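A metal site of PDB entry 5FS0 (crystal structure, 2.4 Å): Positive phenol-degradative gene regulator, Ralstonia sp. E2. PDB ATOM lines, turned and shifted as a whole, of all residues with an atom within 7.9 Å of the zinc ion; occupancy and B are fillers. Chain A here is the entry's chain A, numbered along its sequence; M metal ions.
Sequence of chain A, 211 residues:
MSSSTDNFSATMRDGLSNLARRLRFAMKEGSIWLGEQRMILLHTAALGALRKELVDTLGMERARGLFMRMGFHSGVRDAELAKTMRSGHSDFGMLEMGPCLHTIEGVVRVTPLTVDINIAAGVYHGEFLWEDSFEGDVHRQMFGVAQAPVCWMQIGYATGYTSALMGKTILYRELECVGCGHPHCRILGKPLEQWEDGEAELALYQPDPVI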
ATOM      1  N   VAL A 108     -31.992 -31.496   6.198  1.00  0.00           N
ATOM      2  CA  VAL A 108     -30.945 -30.496   6.304  1.00  0.00           C
ATOM      3  C   VAL A 108     -31.504 -29.289   7.053  1.00  0.00           C
ATOM      4  O   VAL A 108     -32.726 -29.144   7.194  1.00  0.00           O
ATOM      5  CB  VAL A 108     -30.408 -30.072   4.908  1.00  0.00           C
ATOM      6  CG1 VAL A 108     -31.544 -29.606   4.001  1.00  0.00           C
ATOM      7  CG2 VAL A 108     -29.341 -28.978   5.025  1.00  0.00           C
ATOM      8  N   TRP A 130     -26.964 -24.545   3.415  1.00  0.00           N
ATOM      9  CA  TRP A 130     -27.457 -25.866   3.811  1.00  0.00           C
ATOM     10  C   TRP A 130     -26.642 -26.439   4.966  1.00  0.00           C
ATOM     11  O   TRP A 130     -25.786 -27.295   4.755  1.00  0.00           O
ATOM     12  CB  TRP A 130     -27.436 -26.823   2.610  1.00  0.00           C
ATOM     13  CG  TRP A 130     -28.709 -26.832   1.828  1.00  0.00           C
ATOM     14  CD1 TRP A 130     -29.877 -26.201   2.149  1.00  0.00           C
ATOM     15  CD2 TRP A 130     -28.943 -27.513   0.582  1.00  0.00           C
ATOM     16  NE1 TRP A 130     -30.823 -26.438   1.180  1.00  0.00           N
ATOM     17  CE2 TRP A 130     -30.276 -27.248   0.215  1.00  0.00           C
ATOM     18  CE3 TRP A 130     -28.158 -28.317  -0.244  1.00  0.00           C
ATOM     19  CZ2 TRP A 130     -30.834 -27.752  -0.959  1.00  0.00           C
ATOM     20  CZ3 TRP A 130     -28.724 -28.825  -1.404  1.00  0.00           C
ATOM     21  CH2 TRP A 130     -30.048 -28.536  -1.745  1.00  0.00           C
ATOM     22  N   SER A 133     -26.328 -31.230   6.497  1.00  0.00           N
ATOM     23  CA  SER A 133     -26.957 -32.120   5.524  1.00  0.00           C
ATOM     24  C   SER A 133     -26.650 -33.611   5.607  1.00  0.00           C
ATOM     25  O   SER A 133     -25.482 -34.020   5.542  1.00  0.00           O
ATOM     26  CB  SER A 133     -26.549 -31.576   4.160  1.00  0.00           C
ATOM     27  OG  SER A 133     -26.886 -30.205   4.038  1.00  0.00           O
ATOM     28  N   GLU A 135     -27.308 -36.106   3.446  1.00  0.00           N
ATOM     29  CA  GLU A 135     -26.711 -36.578   2.207  1.00  0.00           C
ATOM     30  C   GLU A 135     -25.199 -36.350   2.212  1.00  0.00           C
ATOM     31  O   GLU A 135     -24.430 -37.254   1.857  1.00  0.00           O
ATOM     32  CB  GLU A 135     -27.342 -35.871   1.002  1.00  0.00           C
ATOM     33  CG  GLU A 135     -27.173 -36.614  -0.307  1.00  0.00           C
ATOM     34  CD  GLU A 135     -28.327 -36.373  -1.263  1.00  0.00           C
ATOM     35  OE1 GLU A 135     -29.097 -35.412  -1.042  1.00  0.00           O
ATOM     36  OE2 GLU A 135     -28.470 -37.155  -2.230  1.00  0.00           O
ATOM     37  N   GLY A 136     -24.781 -35.166   2.612  1.00  0.00           N
ATOM     38  CA  GLY A 136     -23.365 -34.829   2.664  1.00  0.00           C
ATOM     39  C   GLY A 136     -22.599 -35.705   3.628  1.00  0.00           C
ATOM     40  O   GLY A 136     -21.537 -36.238   3.285  1.00  0.00           O
ATOM     41  N   ASP A 137     -23.136 -35.869   4.829  1.00  0.00           N
ATOM     42  CA  ASP A 137     -22.488 -36.691   5.854  1.00  0.00           C
ATOM     43  C   ASP A 137     -22.654 -38.177   5.537  1.00  0.00           C
ATOM     44  O   ASP A 137     -21.872 -39.007   6.006  1.00  0.00           O
ATOM     45  CB  ASP A 137     -23.072 -36.380   7.229  1.00  0.00           C
ATOM     46  CG  ASP A 137     -22.828 -34.943   7.656  1.00  0.00           C
ATOM     47  OD1 ASP A 137     -22.114 -34.223   6.933  1.00  0.00           O
ATOM     48  OD2 ASP A 137     -23.353 -34.541   8.717  1.00  0.00           O
ATOM     49  N   ALA A 148     -17.102 -33.817  -6.579  1.00  0.00           N
ATOM     50  CA  ALA A 148     -18.203 -32.890  -6.848  1.00  0.00           C
ATOM     51  C   ALA A 148     -19.300 -33.000  -5.782  1.00  0.00           C
ATOM     52  O   ALA A 148     -19.417 -34.043  -5.126  1.00  0.00           O
ATOM     53  CB  ALA A 148     -18.774 -33.136  -8.239  1.00  0.00           C
ATOM     54  N   PRO A 149     -20.090 -31.926  -5.593  1.00  0.00           N
ATOM     55  CA  PRO A 149     -21.153 -31.860  -4.572  1.00  0.00           C
ATOM     56  C   PRO A 149     -22.070 -33.093  -4.614  1.00  0.00           C
ATOM     57  O   PRO A 149     -22.318 -33.663  -5.672  1.00  0.00           O
ATOM     58  CB  PRO A 149     -21.918 -30.585  -4.936  1.00  0.00           C
ATOM     59  CG  PRO A 149     -20.884 -29.721  -5.591  1.00  0.00           C
ATOM     60  CD  PRO A 149     -20.018 -30.673  -6.375  1.00  0.00           C
ATOM     61  N   VAL A 150     -22.532 -33.511  -3.454  1.00  0.00           N
ATOM     62  CA  VAL A 150     -23.142 -34.837  -3.355  1.00  0.00           C
ATOM     63  C   VAL A 150     -24.574 -34.805  -2.832  1.00  0.00           C
ATOM     64  O   VAL A 150     -25.239 -35.845  -2.774  1.00  0.00           O
ATOM     65  CB  VAL A 150     -22.291 -35.754  -2.451  1.00  0.00           C
ATOM     66  CG1 VAL A 150     -21.040 -36.182  -3.183  1.00  0.00           C
ATOM     67  CG2 VAL A 150     -21.934 -35.052  -1.166  1.00  0.00           C
ATOM     68  N   CYS A 151     -25.055 -33.616  -2.508  1.00  0.00           N
ATOM     69  CA  CYS A 151     -26.425 -33.468  -2.032  1.00  0.00           C
ATOM     70  C   CYS A 151     -27.473 -33.489  -3.170  1.00  0.00           C
ATOM     71  O   CYS A 151     -28.186 -32.522  -3.426  1.00  0.00           O
ATOM     72  CB  CYS A 151     -26.517 -32.203  -1.194  1.00  0.00           C
ATOM     73  SG  CYS A 151     -25.417 -32.304   0.311  1.00  0.00           S
ATOM     74  N   TRP A 152     -27.542 -34.643  -3.832  1.00  0.00           N
ATOM     75  CA  TRP A 152     -28.343 -34.851  -5.032  1.00  0.00           C
ATOM     76  C   TRP A 152     -29.846 -34.745  -4.764  1.00  0.00           C
ATOM     77  O   TRP A 152     -30.573 -33.943  -5.402  1.00  0.00           O
ATOM     78  CB  TRP A 152     -28.034 -36.228  -5.628  1.00  0.00           C
ATOM     79  CG  TRP A 152     -26.552 -36.448  -5.935  1.00  0.00           C
ATOM     80  CD1 TRP A 152     -25.624 -35.476  -6.194  1.00  0.00           C
ATOM     81  CD2 TRP A 152     -25.849 -37.700  -5.999  1.00  0.00           C
ATOM     82  NE1 TRP A 152     -24.398 -36.041  -6.423  1.00  0.00           N
ATOM     83  CE2 TRP A 152     -24.502 -37.410  -6.311  1.00  0.00           C
ATOM     84  CE3 TRP A 152     -26.225 -39.038  -5.823  1.00  0.00           C
ATOM     85  CZ2 TRP A 152     -23.532 -38.403  -6.438  1.00  0.00           C
ATOM     86  CZ3 TRP A 152     -25.259 -40.027  -5.958  1.00  0.00           C
ATOM     87  CH2 TRP A 152     -23.932 -39.706  -6.266  1.00  0.00           C
ATOM     88  N   GLN A 154     -31.249 -33.621  -2.116  1.00  0.00           N
ATOM     89  CA  GLN A 154     -31.539 -32.311  -1.550  1.00  0.00           C
ATOM     90  C   GLN A 154     -31.667 -31.224  -2.612  1.00  0.00           C
ATOM     91  O   GLN A 154     -32.499 -30.326  -2.505  1.00  0.00           O
ATOM     92  CB  GLN A 154     -30.472 -31.942  -0.531  1.00  0.00           C
ATOM     93  CG  GLN A 154     -30.259 -33.030   0.538  1.00  0.00           C
ATOM     94  CD  GLN A 154     -29.277 -32.601   1.630  1.00  0.00           C
ATOM     95  OE1 GLN A 154     -28.709 -31.510   1.555  1.00  0.00           O
ATOM     96  NE2 GLN A 154     -29.090 -33.444   2.640  1.00  0.00           N
ATOM     97  N   ILE A 155     -30.845 -31.331  -3.662  1.00  0.00           N
ATOM     98  CA  ILE A 155     -30.893 -30.400  -4.781  1.00  0.00           C
ATOM     99  C   ILE A 155     -32.124 -30.637  -5.648  1.00  0.00           C
ATOM    100  O   ILE A 155     -32.706 -29.700  -6.194  1.00  0.00           O
ATOM    101  CB  ILE A 155     -29.620 -30.522  -5.650  1.00  0.00           C
ATOM    102  CG1 ILE A 155     -28.538 -29.595  -5.097  1.00  0.00           C
ATOM    103  CG2 ILE A 155     -29.917 -30.167  -7.102  1.00  0.00           C
ATOM    104  CD1 ILE A 155     -28.886 -28.118  -5.207  1.00  0.00           C
ATOM    105  N   GLU A 174     -25.378 -26.660  -6.358  1.00  0.00           N
ATOM    106  CA  GLU A 174     -24.585 -26.405  -5.162  1.00  0.00           C
ATOM    107  C   GLU A 174     -23.317 -25.694  -5.570  1.00  0.00           C
ATOM    108  O   GLU A 174     -22.545 -26.211  -6.367  1.00  0.00           O
ATOM    109  CB  GLU A 174     -24.221 -27.711  -4.428  1.00  0.00           C
ATOM    110  CG  GLU A 174     -25.381 -28.488  -3.844  1.00  0.00           C
ATOM    111  CD  GLU A 174     -24.916 -29.622  -2.944  1.00  0.00           C
ATOM    112  OE1 GLU A 174     -24.637 -29.365  -1.757  1.00  0.00           O
ATOM    113  OE2 GLU A 174     -24.828 -30.770  -3.410  1.00  0.00           O
ATOM    114  N   LEU A 175     -23.106 -24.495  -5.034  1.00  0.00           N
ATOM    115  CA  LEU A 175     -21.869 -23.756  -5.275  1.00  0.00           C
ATOM    116  C   LEU A 175     -20.765 -24.204  -4.313  1.00  0.00           C
ATOM    117  O   LEU A 175     -19.566 -24.012  -4.571  1.00  0.00           O
ATOM    118  CB  LEU A 175     -22.117 -22.257  -5.147  1.00  0.00           C
ATOM    119  CG  LEU A 175     -23.236 -21.690  -6.035  1.00  0.00           C
ATOM    120  CD1 LEU A 175     -23.397 -20.184  -5.831  1.00  0.00           C
ATOM    121  CD2 LEU A 175     -22.991 -22.014  -7.513  1.00  0.00           C
ATOM    122  N   GLU A 176     -21.176 -24.807  -3.199  1.00  0.00           N
ATOM    123  CA  GLU A 176     -20.272 -25.330  -2.177  1.00  0.00           C
ATOM    124  C   GLU A 176     -20.960 -26.452  -1.409  1.00  0.00           C
ATOM    125  O   GLU A 176     -22.161 -26.397  -1.167  1.00  0.00           O
ATOM    126  CB  GLU A 176     -19.813 -24.232  -1.223  1.00  0.00           C
ATOM    127  CG  GLU A 176     -18.794 -23.289  -1.829  1.00  0.00           C
ATOM    128  CD  GLU A 176     -18.658 -21.975  -1.069  1.00  0.00           C
ATOM    129  OE1 GLU A 176     -19.381 -21.785  -0.056  1.00  0.00           O
ATOM    130  OE2 GLU A 176     -17.835 -21.136  -1.506  1.00  0.00           O
ATOM    131  N   CYS A 177     -20.188 -27.468  -1.006  1.00  0.00           N
ATOM    132  CA  CYS A 177     -20.748 -28.692  -0.442  1.00  0.00           C
ATOM    133  C   CYS A 177     -19.817 -29.323   0.597  1.00  0.00           C
ATOM    134  O   CYS A 177     -18.628 -29.484   0.344  1.00  0.00           O
ATOM    135  CB  CYS A 177     -21.033 -29.692  -1.571  1.00  0.00           C
ATOM    136  SG  CYS A 177     -21.858 -31.249  -1.114  1.00  0.00           S
ATOM    137  N   VAL A 178     -20.364 -29.689   1.760  1.00  0.00           N
ATOM    138  CA  VAL A 178     -19.600 -30.433   2.762  1.00  0.00           C
ATOM    139  C   VAL A 178     -19.074 -31.749   2.208  1.00  0.00           C
ATOM    140  O   VAL A 178     -18.118 -32.314   2.736  1.00  0.00           O
ATOM    141  CB  VAL A 178     -20.444 -30.747   4.016  1.00  0.00           C
ATOM    142  CG1 VAL A 178     -20.716 -29.490   4.814  1.00  0.00           C
ATOM    143  CG2 VAL A 178     -21.732 -31.450   3.607  1.00  0.00           C
ATOM    144  N   GLY A 179     -19.717 -32.256   1.170  1.00  0.00           N
ATOM    145  CA  GLY A 179     -19.287 -33.505   0.582  1.00  0.00           C
ATOM    146  C   GLY A 179     -17.958 -33.340  -0.136  1.00  0.00           C
ATOM    147  O   GLY A 179     -17.304 -34.324  -0.482  1.00  0.00           O
ATOM    148  N   CYS A 180     -17.570 -32.095  -0.367  1.00  0.00           N
ATOM    149  CA  CYS A 180     -16.338 -31.790  -1.084  1.00  0.00           C
ATOM    150  C   CYS A 180     -15.291 -31.209  -0.150  1.00  0.00           C
ATOM    151  O   CYS A 180     -14.306 -30.621  -0.593  1.00  0.00           O
ATOM    152  CB  CYS A 180     -16.619 -30.827  -2.240  1.00  0.00           C
ATOM    153  SG  CYS A 180     -17.646 -31.515  -3.562  1.00  0.00           S
ATOM    154  N   HIS A 182     -15.875 -28.836   2.036  1.00  0.00           N
ATOM    155  CA  HIS A 182     -16.313 -27.533   2.519  1.00  0.00           C
ATOM    156  C   HIS A 182     -17.015 -27.654   3.866  1.00  0.00           C
ATOM    157  O   HIS A 182     -17.445 -28.749   4.261  1.00  0.00           O
ATOM    158  CB  HIS A 182     -17.240 -26.853   1.511  1.00  0.00           C
ATOM    159  CG  HIS A 182     -16.610 -26.608   0.181  1.00  0.00           C
ATOM    160  ND1 HIS A 182     -16.361 -27.614  -0.727  1.00  0.00           N
ATOM    161  CD2 HIS A 182     -16.153 -25.467  -0.396  1.00  0.00           C
ATOM    162  CE1 HIS A 182     -15.800 -27.102  -1.812  1.00  0.00           C
ATOM    163  NE2 HIS A 182     -15.661 -25.804  -1.633  1.00  0.00           N
ATOM    164  N   HIS A 184     -19.853 -26.287   4.773  1.00  0.00           N
ATOM    165  CA  HIS A 184     -21.301 -26.377   4.626  1.00  0.00           C
ATOM    166  C   HIS A 184     -21.670 -26.360   3.158  1.00  0.00           C
ATOM    167  O   HIS A 184     -20.796 -26.293   2.290  1.00  0.00           O
ATOM    168  CB  HIS A 184     -21.990 -25.228   5.368  1.00  0.00           C
ATOM    169  CG  HIS A 184     -21.444 -23.873   5.019  1.00  0.00           C
ATOM    170  ND1 HIS A 184     -21.196 -23.478   3.721  1.00  0.00           N
ATOM    171  CD2 HIS A 184     -21.097 -22.826   5.802  1.00  0.00           C
ATOM    172  CE1 HIS A 184     -20.716 -22.252   3.718  1.00  0.00           C
ATOM    173  NE2 HIS A 184     -20.652 -21.836   4.970  1.00  0.00           N
ATOM    174  N   CYS A 185     -22.963 -26.389   2.876  1.00  0.00           N
ATOM    175  CA  CYS A 185     -23.400 -26.315   1.510  1.00  0.00           C
ATOM    176  C   CYS A 185     -23.878 -24.901   1.215  1.00  0.00           C
ATOM    177  O   CYS A 185     -24.349 -24.192   2.096  1.00  0.00           O
ATOM    178  CB  CYS A 185     -24.506 -27.338   1.222  1.00  0.00           C
ATOM    179  SG  CYS A 185     -23.995 -29.068   1.483  1.00  0.00           S
ATOM    180  N   ARG A 186     -23.707 -24.495  -0.034  1.00  0.00           N
ATOM    181  CA  ARG A 186     -24.170 -23.209  -0.501  1.00  0.00           C
ATOM    182  C   ARG A 186     -24.839 -23.483  -1.832  1.00  0.00           C
ATOM    183  O   ARG A 186     -24.248 -24.134  -2.699  1.00  0.00           O
ATOM    184  CB  ARG A 186     -22.996 -22.227  -0.637  1.00  0.00           C
ATOM    185  CG  ARG A 186     -23.377 -20.787  -0.714  1.00  0.00           C
ATOM    186  CD  ARG A 186     -22.349 -19.982  -1.485  1.00  0.00           C
ATOM    187  NE  ARG A 186     -22.893 -18.673  -1.854  1.00  0.00           N
ATOM    188  CZ  ARG A 186     -22.398 -17.894  -2.815  1.00  0.00           C
ATOM    189  NH1 ARG A 186     -21.342 -18.283  -3.521  1.00  0.00           N
ATOM    190  NH2 ARG A 186     -22.974 -16.719  -3.072  1.00  0.00           N
ATOM    191  N   ILE A 187     -26.070 -23.028  -2.019  1.00  0.00           N
ATOM    192  CA  ILE A 187     -26.783 -23.368  -3.250  1.00  0.00           C
ATOM    193  C   ILE A 187     -27.408 -22.153  -3.929  1.00  0.00           C
ATOM    194  O   ILE A 187     -27.781 -21.171  -3.274  1.00  0.00           O
ATOM    195  CB  ILE A 187     -27.912 -24.421  -3.002  1.00  0.00           C
ATOM    196  CG1 ILE A 187     -29.225 -23.717  -2.658  1.00  0.00           C
ATOM    197  CG2 ILE A 187     -27.481 -25.469  -1.932  1.00  0.00           C
ATOM    198  CD1 ILE A 187     -30.433 -24.645  -2.627  1.00  0.00           C
HETATM  199 ZN    ZN M   1     -23.982 -30.556  -0.164  1.00  0.00          ZN
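The side-chain sulfur (SG) of Cys 177 sits close to the backbone NH (N) of Val 150. O of Cys 185 is in hydrogen-bond range of N of Trp 130, 3.0 Å away. OE1 of Gln 154 lies close to SG of Cys 151 (3.6 Å). The backbone NH of Gly 136 lies close to the side-chain sulfur of Cys 151. ND1 of His 182 lies within hydrogen-bond range of O of Cys 177 (3.1 Å). N of Gly 179 lies close to SG of Cys 177. N of Val 178 lies close to SG of Cys 185 (3.7 Å).
Of the 25 residues printed, 4 come within 4 Å of the zinc ion. The nearest printed residue that does not touch the zinc ion is Val 178 (4.2 Å).
The zinc ion is bound by the side-chain carboxylate of Glu 174 (2.1 Å), the side-chain sulfur of Cys 185 (2.2 Å), the side-chain sulfur of Cys 151 (2.3 Å) and the side-chain sulfur of Cys 177 (2.4 Å).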
